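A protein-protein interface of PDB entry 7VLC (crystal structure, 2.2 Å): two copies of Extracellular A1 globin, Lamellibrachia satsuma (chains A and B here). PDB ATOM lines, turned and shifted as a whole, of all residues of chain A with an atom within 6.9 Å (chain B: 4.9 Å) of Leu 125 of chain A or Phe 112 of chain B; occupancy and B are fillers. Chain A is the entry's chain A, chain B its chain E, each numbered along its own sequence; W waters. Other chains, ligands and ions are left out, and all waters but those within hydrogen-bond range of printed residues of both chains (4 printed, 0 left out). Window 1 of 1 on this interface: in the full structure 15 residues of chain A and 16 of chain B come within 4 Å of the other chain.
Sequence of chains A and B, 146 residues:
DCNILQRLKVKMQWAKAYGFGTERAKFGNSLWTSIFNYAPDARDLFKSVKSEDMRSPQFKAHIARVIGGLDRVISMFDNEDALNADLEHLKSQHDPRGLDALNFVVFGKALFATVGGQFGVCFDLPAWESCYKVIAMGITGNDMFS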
ATOM      1  N   GLN A  13      -3.588  12.387 -18.251  1.00  0.00           N
ATOM      2  CA  GLN A  13      -4.349  13.441 -17.593  1.00  0.00           C
ATOM      3  C   GLN A  13      -5.780  13.510 -18.110  1.00  0.00           C
ATOM      4  O   GLN A  13      -6.689  13.864 -17.352  1.00  0.00           O
ATOM      5  CB  GLN A  13      -3.633  14.775 -17.774  1.00  0.00           C
ATOM      6  CG  GLN A  13      -2.197  14.755 -17.268  1.00  0.00           C
ATOM      7  CD  GLN A  13      -1.556  16.125 -17.291  1.00  0.00           C
ATOM      8  OE1 GLN A  13      -2.040  17.035 -17.963  1.00  0.00           O
ATOM      9  NE2 GLN A  13      -0.459  16.282 -16.554  1.00  0.00           N
ATOM     10  N   GLY A 108      -9.789  24.934 -27.755  1.00  0.00           N
ATOM     11  CA  GLY A 108      -8.610  24.464 -27.045  1.00  0.00           C
ATOM     12  C   GLY A 108      -8.429  25.144 -25.701  1.00  0.00           C
ATOM     13  O   GLY A 108      -8.182  24.485 -24.688  1.00  0.00           O
ATOM     14  N   PHE A 112      -8.318  23.283 -22.138  1.00  0.00           N
ATOM     15  CA  PHE A 112      -7.216  23.359 -21.180  1.00  0.00           C
ATOM     16  C   PHE A 112      -7.709  23.814 -19.813  1.00  0.00           C
ATOM     17  O   PHE A 112      -7.291  23.276 -18.782  1.00  0.00           O
ATOM     18  CB  PHE A 112      -6.125  24.312 -21.683  1.00  0.00           C
ATOM     19  CG  PHE A 112      -5.675  24.046 -23.094  1.00  0.00           C
ATOM     20  CD1 PHE A 112      -5.663  22.755 -23.607  1.00  0.00           C
ATOM     21  CD2 PHE A 112      -5.270  25.090 -23.909  1.00  0.00           C
ATOM     22  CE1 PHE A 112      -5.257  22.513 -24.909  1.00  0.00           C
ATOM     23  CE2 PHE A 112      -4.863  24.857 -25.212  1.00  0.00           C
ATOM     24  CZ  PHE A 112      -4.855  23.564 -25.711  1.00  0.00           C
ATOM     25  N   ALA A 113      -8.596  24.808 -19.784  1.00  0.00           N
ATOM     26  CA  ALA A 113      -9.112  25.298 -18.511  1.00  0.00           C
ATOM     27  C   ALA A 113      -9.944  24.235 -17.808  1.00  0.00           C
ATOM     28  O   ALA A 113      -9.897  24.114 -16.577  1.00  0.00           O
ATOM     29  CB  ALA A 113      -9.934  26.567 -18.730  1.00  0.00           C
ATOM     30  N   CYS A 122      -0.753  19.701 -11.436  1.00  0.00           N
ATOM     31  CA  CYS A 122       0.199  18.958 -12.254  1.00  0.00           C
ATOM     32  C   CYS A 122      -0.202  18.913 -13.728  1.00  0.00           C
ATOM     33  O   CYS A 122       0.427  18.193 -14.513  1.00  0.00           O
ATOM     34  CB  CYS A 122       0.368  17.543 -11.696  1.00  0.00           C
ATOM     35  SG  CYS A 122       0.831  17.518  -9.930  1.00  0.00           S
ATOM     36  N   PHE A 123      -1.227  19.668 -14.108  1.00  0.00           N
ATOM     37  CA  PHE A 123      -1.625  19.774 -15.503  1.00  0.00           C
ATOM     38  C   PHE A 123      -0.450  20.246 -16.350  1.00  0.00           C
ATOM     39  O   PHE A 123       0.210  21.239 -16.023  1.00  0.00           O
ATOM     40  CB  PHE A 123      -2.805  20.741 -15.605  1.00  0.00           C
ATOM     41  CG  PHE A 123      -3.297  20.983 -17.004  1.00  0.00           C
ATOM     42  CD1 PHE A 123      -3.907  19.968 -17.723  1.00  0.00           C
ATOM     43  CD2 PHE A 123      -3.201  22.241 -17.577  1.00  0.00           C
ATOM     44  CE1 PHE A 123      -4.385  20.192 -19.003  1.00  0.00           C
ATOM     45  CE2 PHE A 123      -3.679  22.474 -18.859  1.00  0.00           C
ATOM     46  CZ  PHE A 123      -4.271  21.443 -19.573  1.00  0.00           C
ATOM     47  N   ASP A 124      -0.167  19.507 -17.427  1.00  0.00           N
ATOM     48  CA  ASP A 124       0.940  19.825 -18.332  1.00  0.00           C
ATOM     49  C   ASP A 124       0.379  20.648 -19.482  1.00  0.00           C
ATOM     50  O   ASP A 124      -0.002  20.118 -20.527  1.00  0.00           O
ATOM     51  CB  ASP A 124       1.619  18.549 -18.826  1.00  0.00           C
ATOM     52  CG  ASP A 124       2.953  18.813 -19.518  1.00  0.00           C
ATOM     53  OD1 ASP A 124       3.135  19.901 -20.122  1.00  0.00           O
ATOM     54  OD2 ASP A 124       3.817  17.918 -19.464  1.00  0.00           O
ATOM     55  N   LEU A 125       0.337  21.965 -19.291  1.00  0.00           N
ATOM     56  CA  LEU A 125      -0.216  22.838 -20.324  1.00  0.00           C
ATOM     57  C   LEU A 125       0.577  22.825 -21.635  1.00  0.00           C
ATOM     58  O   LEU A 125      -0.061  22.760 -22.701  1.00  0.00           O
ATOM     59  CB  LEU A 125      -0.358  24.262 -19.769  1.00  0.00           C
ATOM     60  CG  LEU A 125      -0.900  25.317 -20.737  1.00  0.00           C
ATOM     61  CD1 LEU A 125      -2.281  24.927 -21.266  1.00  0.00           C
ATOM     62  CD2 LEU A 125      -0.947  26.677 -20.065  1.00  0.00           C
ATOM     63  N   PRO A 126       1.918  22.909 -21.649  1.00  0.00           N
ATOM     64  CA  PRO A 126       2.631  22.812 -22.942  1.00  0.00           C
ATOM     65  C   PRO A 126       2.297  21.553 -23.727  1.00  0.00           C
ATOM     66  O   PRO A 126       2.125  21.616 -24.953  1.00  0.00           O
ATOM     67  CB  PRO A 126       4.107  22.846 -22.529  1.00  0.00           C
ATOM     68  CG  PRO A 126       4.107  23.621 -21.239  1.00  0.00           C
ATOM     69  CD  PRO A 126       2.843  23.215 -20.541  1.00  0.00           C
ATOM     70  N   ALA A 127       2.192  20.406 -23.049  1.00  0.00           N
ATOM     71  CA  ALA A 127       1.871  19.164 -23.741  1.00  0.00           C
ATOM     72  C   ALA A 127       0.475  19.212 -24.351  1.00  0.00           C
ATOM     73  O   ALA A 127       0.267  18.741 -25.476  1.00  0.00           O
ATOM     74  CB  ALA A 127       1.999  17.985 -22.780  1.00  0.00           C
ATOM     75  N   TRP A 128      -0.494  19.789 -23.628  1.00  0.00           N
ATOM     76  CA  TRP A 128      -1.856  19.863 -24.146  1.00  0.00           C
ATOM     77  C   TRP A 128      -1.965  20.854 -25.304  1.00  0.00           C
ATOM     78  O   TRP A 128      -2.699  20.606 -26.266  1.00  0.00           O
ATOM     79  CB  TRP A 128      -2.822  20.227 -23.023  1.00  0.00           C
ATOM     80  CG  TRP A 128      -3.211  19.051 -22.181  1.00  0.00           C
ATOM     81  CD1 TRP A 128      -2.521  18.535 -21.118  1.00  0.00           C
ATOM     82  CD2 TRP A 128      -4.373  18.234 -22.339  1.00  0.00           C
ATOM     83  NE1 TRP A 128      -3.187  17.452 -20.602  1.00  0.00           N
ATOM     84  CE2 TRP A 128      -4.329  17.247 -21.333  1.00  0.00           C
ATOM     85  CE3 TRP A 128      -5.451  18.241 -23.232  1.00  0.00           C
ATOM     86  CZ2 TRP A 128      -5.313  16.277 -21.199  1.00  0.00           C
ATOM     87  CZ3 TRP A 128      -6.429  17.282 -23.093  1.00  0.00           C
ATOM     88  CH2 TRP A 128      -6.353  16.310 -22.082  1.00  0.00           C
ATOM     89  N   GLU A 129      -1.250  21.979 -25.229  1.00  0.00           N
ATOM     90  CA  GLU A 129      -1.228  22.915 -26.352  1.00  0.00           C
ATOM     91  C   GLU A 129      -0.680  22.250 -27.612  1.00  0.00           C
ATOM     92  O   GLU A 129      -1.256  22.382 -28.698  1.00  0.00           O
ATOM     93  CB  GLU A 129      -0.398  24.146 -25.993  1.00  0.00           C
ATOM     94  CG  GLU A 129      -1.032  25.051 -24.953  1.00  0.00           C
ATOM     95  CD  GLU A 129      -0.125  26.211 -24.587  1.00  0.00           C
ATOM     96  OE1 GLU A 129       1.103  26.073 -24.766  1.00  0.00           O
ATOM     97  OE2 GLU A 129      -0.629  27.260 -24.138  1.00  0.00           O
ATOM     98  N   SER A 130       0.435  21.525 -27.483  1.00  0.00           N
ATOM     99  CA  SER A 130       1.048  20.881 -28.643  1.00  0.00           C
ATOM    100  C   SER A 130       0.163  19.778 -29.211  1.00  0.00           C
ATOM    101  O   SER A 130       0.020  19.661 -30.432  1.00  0.00           O
ATOM    102  CB  SER A 130       2.417  20.316 -28.269  1.00  0.00           C
ATOM    103  OG  SER A 130       3.270  21.336 -27.786  1.00  0.00           O
ATOM    104  N   CYS A 131      -0.432  18.956 -28.347  1.00  0.00           N
ATOM    105  CA  CYS A 131      -1.205  17.818 -28.827  1.00  0.00           C
ATOM    106  C   CYS A 131      -2.617  18.205 -29.259  1.00  0.00           C
ATOM    107  O   CYS A 131      -3.207  17.507 -30.092  1.00  0.00           O
ATOM    108  CB  CYS A 131      -1.236  16.720 -27.760  1.00  0.00           C
ATOM    109  SG  CYS A 131       0.375  15.880 -27.560  1.00  0.00           S
ATOM    110  N   TYR B  38       8.752  21.728 -16.833  1.00  0.00           N
ATOM    111  CA  TYR B  38       8.537  22.183 -18.205  1.00  0.00           C
ATOM    112  C   TYR B  38       9.853  22.444 -18.926  1.00  0.00           C
ATOM    113  O   TYR B  38       9.944  22.227 -20.139  1.00  0.00           O
ATOM    114  CB  TYR B  38       7.685  23.456 -18.229  1.00  0.00           C
ATOM    115  CG  TYR B  38       6.223  23.266 -17.890  1.00  0.00           C
ATOM    116  CD1 TYR B  38       5.681  21.997 -17.733  1.00  0.00           C
ATOM    117  CD2 TYR B  38       5.380  24.363 -17.743  1.00  0.00           C
ATOM    118  CE1 TYR B  38       4.345  21.828 -17.423  1.00  0.00           C
ATOM    119  CE2 TYR B  38       4.048  24.202 -17.436  1.00  0.00           C
ATOM    120  CZ  TYR B  38       3.536  22.935 -17.275  1.00  0.00           C
ATOM    121  OH  TYR B  38       2.205  22.786 -16.972  1.00  0.00           O
ATOM    122  N   GLY B 108       4.968  31.621 -17.723  1.00  0.00           N
ATOM    123  CA  GLY B 108       3.540  31.838 -17.881  1.00  0.00           C
ATOM    124  C   GLY B 108       2.753  30.543 -17.939  1.00  0.00           C
ATOM    125  O   GLY B 108       1.687  30.429 -17.328  1.00  0.00           O
ATOM    126  N   LYS B 109       3.263  29.551 -18.677  1.00  0.00           N
ATOM    127  CA  LYS B 109       2.570  28.268 -18.771  1.00  0.00           C
ATOM    128  C   LYS B 109       2.455  27.610 -17.401  1.00  0.00           C
ATOM    129  O   LYS B 109       1.405  27.061 -17.052  1.00  0.00           O
ATOM    130  CB  LYS B 109       3.296  27.340 -19.750  1.00  0.00           C
ATOM    131  CG  LYS B 109       2.796  27.386 -21.202  1.00  0.00           C
ATOM    132  CD  LYS B 109       3.261  28.626 -21.938  1.00  0.00           C
ATOM    133  CE  LYS B 109       2.797  28.633 -23.395  1.00  0.00           C
ATOM    134  NZ  LYS B 109       3.309  27.459 -24.152  1.00  0.00           N
ATOM    135  N   ALA B 110       3.522  27.661 -16.607  1.00  0.00           N
ATOM    136  CA  ALA B 110       3.468  27.074 -15.274  1.00  0.00           C
ATOM    137  C   ALA B 110       2.518  27.849 -14.372  1.00  0.00           C
ATOM    138  O   ALA B 110       1.777  27.252 -13.584  1.00  0.00           O
ATOM    139  CB  ALA B 110       4.869  27.027 -14.667  1.00  0.00           C
ATOM    140  N   LEU B 111       2.523  29.181 -14.483  1.00  0.00           N
ATOM    141  CA  LEU B 111       1.597  29.994 -13.706  1.00  0.00           C
ATOM    142  C   LEU B 111       0.144  29.661 -14.039  1.00  0.00           C
ATOM    143  O   LEU B 111      -0.699  29.584 -13.141  1.00  0.00           O
ATOM    144  CB  LEU B 111       1.876  31.476 -13.943  1.00  0.00           C
ATOM    145  CG  LEU B 111       0.951  32.456 -13.213  1.00  0.00           C
ATOM    146  CD1 LEU B 111       1.153  32.385 -11.697  1.00  0.00           C
ATOM    147  CD2 LEU B 111       1.151  33.876 -13.738  1.00  0.00           C
ATOM    148  N   PHE B 112      -0.169  29.456 -15.326  1.00  0.00           N
ATOM    149  CA  PHE B 112      -1.547  29.136 -15.703  1.00  0.00           C
ATOM    150  C   PHE B 112      -1.966  27.774 -15.164  1.00  0.00           C
ATOM    151  O   PHE B 112      -3.080  27.620 -14.652  1.00  0.00           O
ATOM    152  CB  PHE B 112      -1.718  29.172 -17.226  1.00  0.00           C
ATOM    153  CG  PHE B 112      -1.265  30.456 -17.861  1.00  0.00           C
ATOM    154  CD1 PHE B 112      -1.337  31.653 -17.164  1.00  0.00           C
ATOM    155  CD2 PHE B 112      -0.756  30.460 -19.151  1.00  0.00           C
ATOM    156  CE1 PHE B 112      -0.906  32.832 -17.741  1.00  0.00           C
ATOM    157  CE2 PHE B 112      -0.324  31.638 -19.734  1.00  0.00           C
ATOM    158  CZ  PHE B 112      -0.400  32.828 -19.029  1.00  0.00           C
ATOM    159  N   ALA B 113      -1.090  26.772 -15.279  1.00  0.00           N
ATOM    160  CA  ALA B 113      -1.421  25.442 -14.778  1.00  0.00           C
ATOM    161  C   ALA B 113      -1.565  25.424 -13.261  1.00  0.00           C
ATOM    162  O   ALA B 113      -2.376  24.658 -12.729  1.00  0.00           O
ATOM    163  CB  ALA B 113      -0.359  24.436 -15.214  1.00  0.00           C
ATOM    164  N   THR B 114      -0.782  26.246 -12.554  1.00  0.00           N
ATOM    165  CA  THR B 114      -0.836  26.267 -11.095  1.00  0.00           C
ATOM    166  C   THR B 114      -2.082  26.988 -10.605  1.00  0.00           C
ATOM    167  O   THR B 114      -2.830  26.456  -9.778  1.00  0.00           O
ATOM    168  CB  THR B 114       0.416  26.933 -10.522  1.00  0.00           C
ATOM    169  OG1 THR B 114       1.584  26.323 -11.088  1.00  0.00           O
ATOM    170  CG2 THR B 114       0.454  26.775  -9.004  1.00  0.00           C
ATOM    171  N   VAL B 115      -2.324  28.199 -11.114  1.00  0.00           N
ATOM    172  CA  VAL B 115      -3.522  28.935 -10.720  1.00  0.00           C
ATOM    173  C   VAL B 115      -4.772  28.190 -11.173  1.00  0.00           C
ATOM    174  O   VAL B 115      -5.711  27.993 -10.397  1.00  0.00           O
ATOM    175  CB  VAL B 115      -3.490  30.370 -11.276  1.00  0.00           C
ATOM    176  CG1 VAL B 115      -4.786  31.095 -10.926  1.00  0.00           C
ATOM    177  CG2 VAL B 115      -2.293  31.134 -10.730  1.00  0.00           C
ATOM    178  N   GLY B 116      -4.795  27.758 -12.439  1.00  0.00           N
ATOM    179  CA  GLY B 116      -5.940  27.007 -12.933  1.00  0.00           C
ATOM    180  C   GLY B 116      -6.176  25.719 -12.168  1.00  0.00           C
ATOM    181  O   GLY B 116      -7.314  25.395 -11.813  1.00  0.00           O
ATOM    182  N   GLY B 117      -5.101  24.967 -11.897  1.00  0.00           N
ATOM    183  CA  GLY B 117      -5.236  23.727 -11.152  1.00  0.00           C
ATOM    184  C   GLY B 117      -5.779  23.935  -9.754  1.00  0.00           C
ATOM    185  O   GLY B 117      -6.495  23.078  -9.226  1.00  0.00           O
ATOM    186  N   PHE B 123     -11.401  28.749 -14.422  1.00  0.00           N
ATOM    187  CA  PHE B 123     -10.199  29.512 -14.735  1.00  0.00           C
ATOM    188  C   PHE B 123     -10.311  30.103 -16.138  1.00  0.00           C
ATOM    189  O   PHE B 123     -10.656  29.402 -17.093  1.00  0.00           O
ATOM    190  CB  PHE B 123      -8.980  28.591 -14.622  1.00  0.00           C
ATOM    191  CG  PHE B 123      -7.668  29.242 -14.962  1.00  0.00           C
ATOM    192  CD1 PHE B 123      -7.101  30.168 -14.107  1.00  0.00           C
ATOM    193  CD2 PHE B 123      -6.976  28.888 -16.118  1.00  0.00           C
ATOM    194  CE1 PHE B 123      -5.886  30.759 -14.399  1.00  0.00           C
ATOM    195  CE2 PHE B 123      -5.752  29.478 -16.421  1.00  0.00           C
ATOM    196  CZ  PHE B 123      -5.208  30.417 -15.557  1.00  0.00           C
ATOM    197  N   LEU B 125      -8.454  31.123 -18.928  1.00  0.00           N
ATOM    198  CA  LEU B 125      -7.140  31.047 -19.558  1.00  0.00           C
ATOM    199  C   LEU B 125      -6.872  32.174 -20.556  1.00  0.00           C
ATOM    200  O   LEU B 125      -5.757  32.724 -20.528  1.00  0.00           O
ATOM    201  CB  LEU B 125      -6.966  29.671 -20.218  1.00  0.00           C
ATOM    202  CG  LEU B 125      -5.659  29.441 -20.977  1.00  0.00           C
ATOM    203  CD1 LEU B 125      -4.471  29.641 -20.050  1.00  0.00           C
ATOM    204  CD2 LEU B 125      -5.631  28.052 -21.603  1.00  0.00           C
ATOM    205  N   TRP B 128      -5.895  35.269 -18.521  1.00  0.00           N
ATOM    206  CA  TRP B 128      -4.573  35.159 -17.912  1.00  0.00           C
ATOM    207  C   TRP B 128      -3.463  35.243 -18.958  1.00  0.00           C
ATOM    208  O   TRP B 128      -2.409  35.831 -18.698  1.00  0.00           O
ATOM    209  CB  TRP B 128      -4.476  33.858 -17.117  1.00  0.00           C
ATOM    210  CG  TRP B 128      -5.006  33.989 -15.723  1.00  0.00           C
ATOM    211  CD1 TRP B 128      -6.302  33.852 -15.319  1.00  0.00           C
ATOM    212  CD2 TRP B 128      -4.249  34.294 -14.547  1.00  0.00           C
ATOM    213  NE1 TRP B 128      -6.399  34.049 -13.960  1.00  0.00           N
ATOM    214  CE2 TRP B 128      -5.152  34.320 -13.463  1.00  0.00           C
ATOM    215  CE3 TRP B 128      -2.896  34.550 -14.304  1.00  0.00           C
ATOM    216  CZ2 TRP B 128      -4.744  34.593 -12.159  1.00  0.00           C
ATOM    217  CZ3 TRP B 128      -2.494  34.820 -13.011  1.00  0.00           C
ATOM    218  CH2 TRP B 128      -3.414  34.841 -11.953  1.00  0.00           C
ATOM    219  N   GLU B 129      -3.676  34.658 -20.139  1.00  0.00           N
ATOM    220  CA  GLU B 129      -2.680  34.755 -21.205  1.00  0.00           C
ATOM    221  C   GLU B 129      -2.427  36.207 -21.583  1.00  0.00           C
ATOM    222  O   GLU B 129      -1.273  36.653 -21.661  1.00  0.00           O
ATOM    223  CB  GLU B 129      -3.136  33.958 -22.429  1.00  0.00           C
ATOM    224  CG  GLU B 129      -2.989  32.446 -22.298  1.00  0.00           C
ATOM    225  CD  GLU B 129      -3.531  31.701 -23.509  1.00  0.00           C
ATOM    226  OE1 GLU B 129      -4.320  32.302 -24.263  1.00  0.00           O
ATOM    227  OE2 GLU B 129      -3.171  30.516 -23.709  1.00  0.00           O
ATOM    228  N   TYR B 132      -0.872  38.167 -18.484  1.00  0.00           N
ATOM    229  CA  TYR B 132       0.508  37.812 -18.182  1.00  0.00           C
ATOM    230  C   TYR B 132       1.459  38.420 -19.198  1.00  0.00           C
ATOM    231  O   TYR B 132       2.594  38.774 -18.851  1.00  0.00           O
ATOM    232  CB  TYR B 132       0.695  36.300 -18.131  1.00  0.00           C
ATOM    233  CG  TYR B 132       2.137  35.917 -17.905  1.00  0.00           C
ATOM    234  CD1 TYR B 132       2.703  35.974 -16.636  1.00  0.00           C
ATOM    235  CD2 TYR B 132       2.942  35.521 -18.967  1.00  0.00           C
ATOM    236  CE1 TYR B 132       4.028  35.635 -16.432  1.00  0.00           C
ATOM    237  CE2 TYR B 132       4.260  35.183 -18.777  1.00  0.00           C
ATOM    238  CZ  TYR B 132       4.802  35.238 -17.506  1.00  0.00           C
ATOM    239  OH  TYR B 132       6.119  34.900 -17.326  1.00  0.00           O
HETATM  240  O   HOH W   1      -8.252  25.487 -15.081  1.00  0.00           O
HETATM  241  O   HOH W   2      -3.194  28.132 -24.587  1.00  0.00           O
HETATM  242  O   HOH W   3      -0.840  29.389 -22.962  1.00  0.00           O
HETATM  243  O   HOH W   4       2.491  21.306 -14.413  1.00  0.00           O
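The backbone carbonyl oxygen of Phe 123 of chain A lies within hydrogen-bond range of the side-chain hydroxyl of Tyr 38 of chain B, at 2.7 Å. N of Leu 125 of chain A is in hydrogen-bond range of OH of Tyr 38 of chain B. The side-chain amino group (NZ) of Lys 109 of chain B lies within salt-bridge range of the side-chain carboxylate (OE1) of Glu 129 of chain A, at 2.7 Å.
Of the 16 printed residues of chain B, 6 touch a printed residue of chain A. Hydrophobic or aromatic side chains of chain B within 4 Å of the printed part of chain A: Tyr 38, Phe 112, Ala 113 and Leu 125. Hydrophobic or aromatic side chains of chain A that line the printed part of chain B: Phe 112, Ala 113, Leu 125 and Pro 126. Along chain A the printed residues that touch a printed residue of chain B span positions 112 to 129. Among the printed residues, Asp or Glu carboxylates within 4 Å of a Lys or Arg side-chain nitrogen of the other chain: Glu 129 of chain A with Lys 109 of chain B.
OE1 of Gln 13 of chain A is in hydrogen-bond range of N of Asp 124 of chain A, at 3.1 Å. N of Ala 127 of chain A lies within hydrogen-bond range of OD1 of Asp 124 of chain A (3.1 Å). The side-chain hydroxyl (OG) of Ser 130 of chain A sits at hydrogen-bond distance from the backbone carbonyl oxygen (O) of Pro 126 of chain A (3.1 Å).
Printed residues of chain B within 4 Å of Phe 112 of chain A: Leu 125 (3.8 Å). Leu 125 of chain A touches three residues of chain B. Of the printed residues of chain B, Glu 129 of chain A touches Lys 109 (2.7 Å). Printed residues of chain A within 4 Å of Tyr 38 of chain B: Phe 123, Asp 124, Leu 125 and Pro 126. Of the printed residues of chain A, Lys 109 of chain B touches Leu 125 (3.8 Å), Pro 126 (3.99 Å) and Glu 129 (2.7 Å). Phe 112 of chain B touches just one residue of chain A: Leu 125. Of the printed residues of chain A, Leu 125 of chain B touches Phe 112. Glu 129 of chain B touches none of the printed residues of chain A. The nearest residue of chain B that does not touch Leu 125 of chain A is Ala 113 of chain B (4.6 Å). The nearest printed residue of chain B that does not touch Pro 126 of chain A is Ala 110 of chain B (6.0 Å).
Among the printed residues, pairs that only touch across the chains: Phe 112 of chain A with Leu 125 of chain B (3.8 Å), Ala 113 of chain A with Phe 123 of chain B (3.4 Å), Phe 123 of chain A with Ala 113 of chain B (3.3 Å), Asp 124 of chain A with Tyr 38 of chain B (3.5 Å), Leu 125 of chain A with Lys 109 of chain B (3.8 Å), Leu 125 of chain A with Phe 112 of chain B (3.9 Å), Pro 126 of chain A with Tyr 38 of chain B (3.4 Å) and Pro 126 of chain A with Lys 109 of chain B (3.99 Å).
Water W3 lies within hydrogen-bond range of OE2 of Glu 129 of chain A (2.4 Å) and OE2 of Glu 129 of chain B (2.7 Å). Water W2 bridges the side-chain carboxylate (OE2) of Glu 129 of chain B (2.5 Å) and the side-chain carboxylate (OE2) of Glu 129 of chain A (2.7 Å). Water W1 lies within hydrogen-bond range of the backbone carbonyl oxygen (O) of Ala 113 of chain A (2.6 Å) and the backbone carbonyl oxygen (O) of Gly 116 of chain B (3.4 Å). Water W4 bridges O of Phe 123 of chain A (2.8 Å) and OH of Tyr 38 of chain B (3.0 Å).
Phe 112 of chain A touches Leu 125 of chain B, and with the chains exchanged Leu 125 of chain A touches Phe 112 of chain B. Ala 113 of chain A touches Phe 123 of chain B, and with the chains exchanged Phe 123 of chain A touches Ala 113 of chain B. Positions printed for both chains: 108, 112, 113, 123, 125, 128 and 129.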
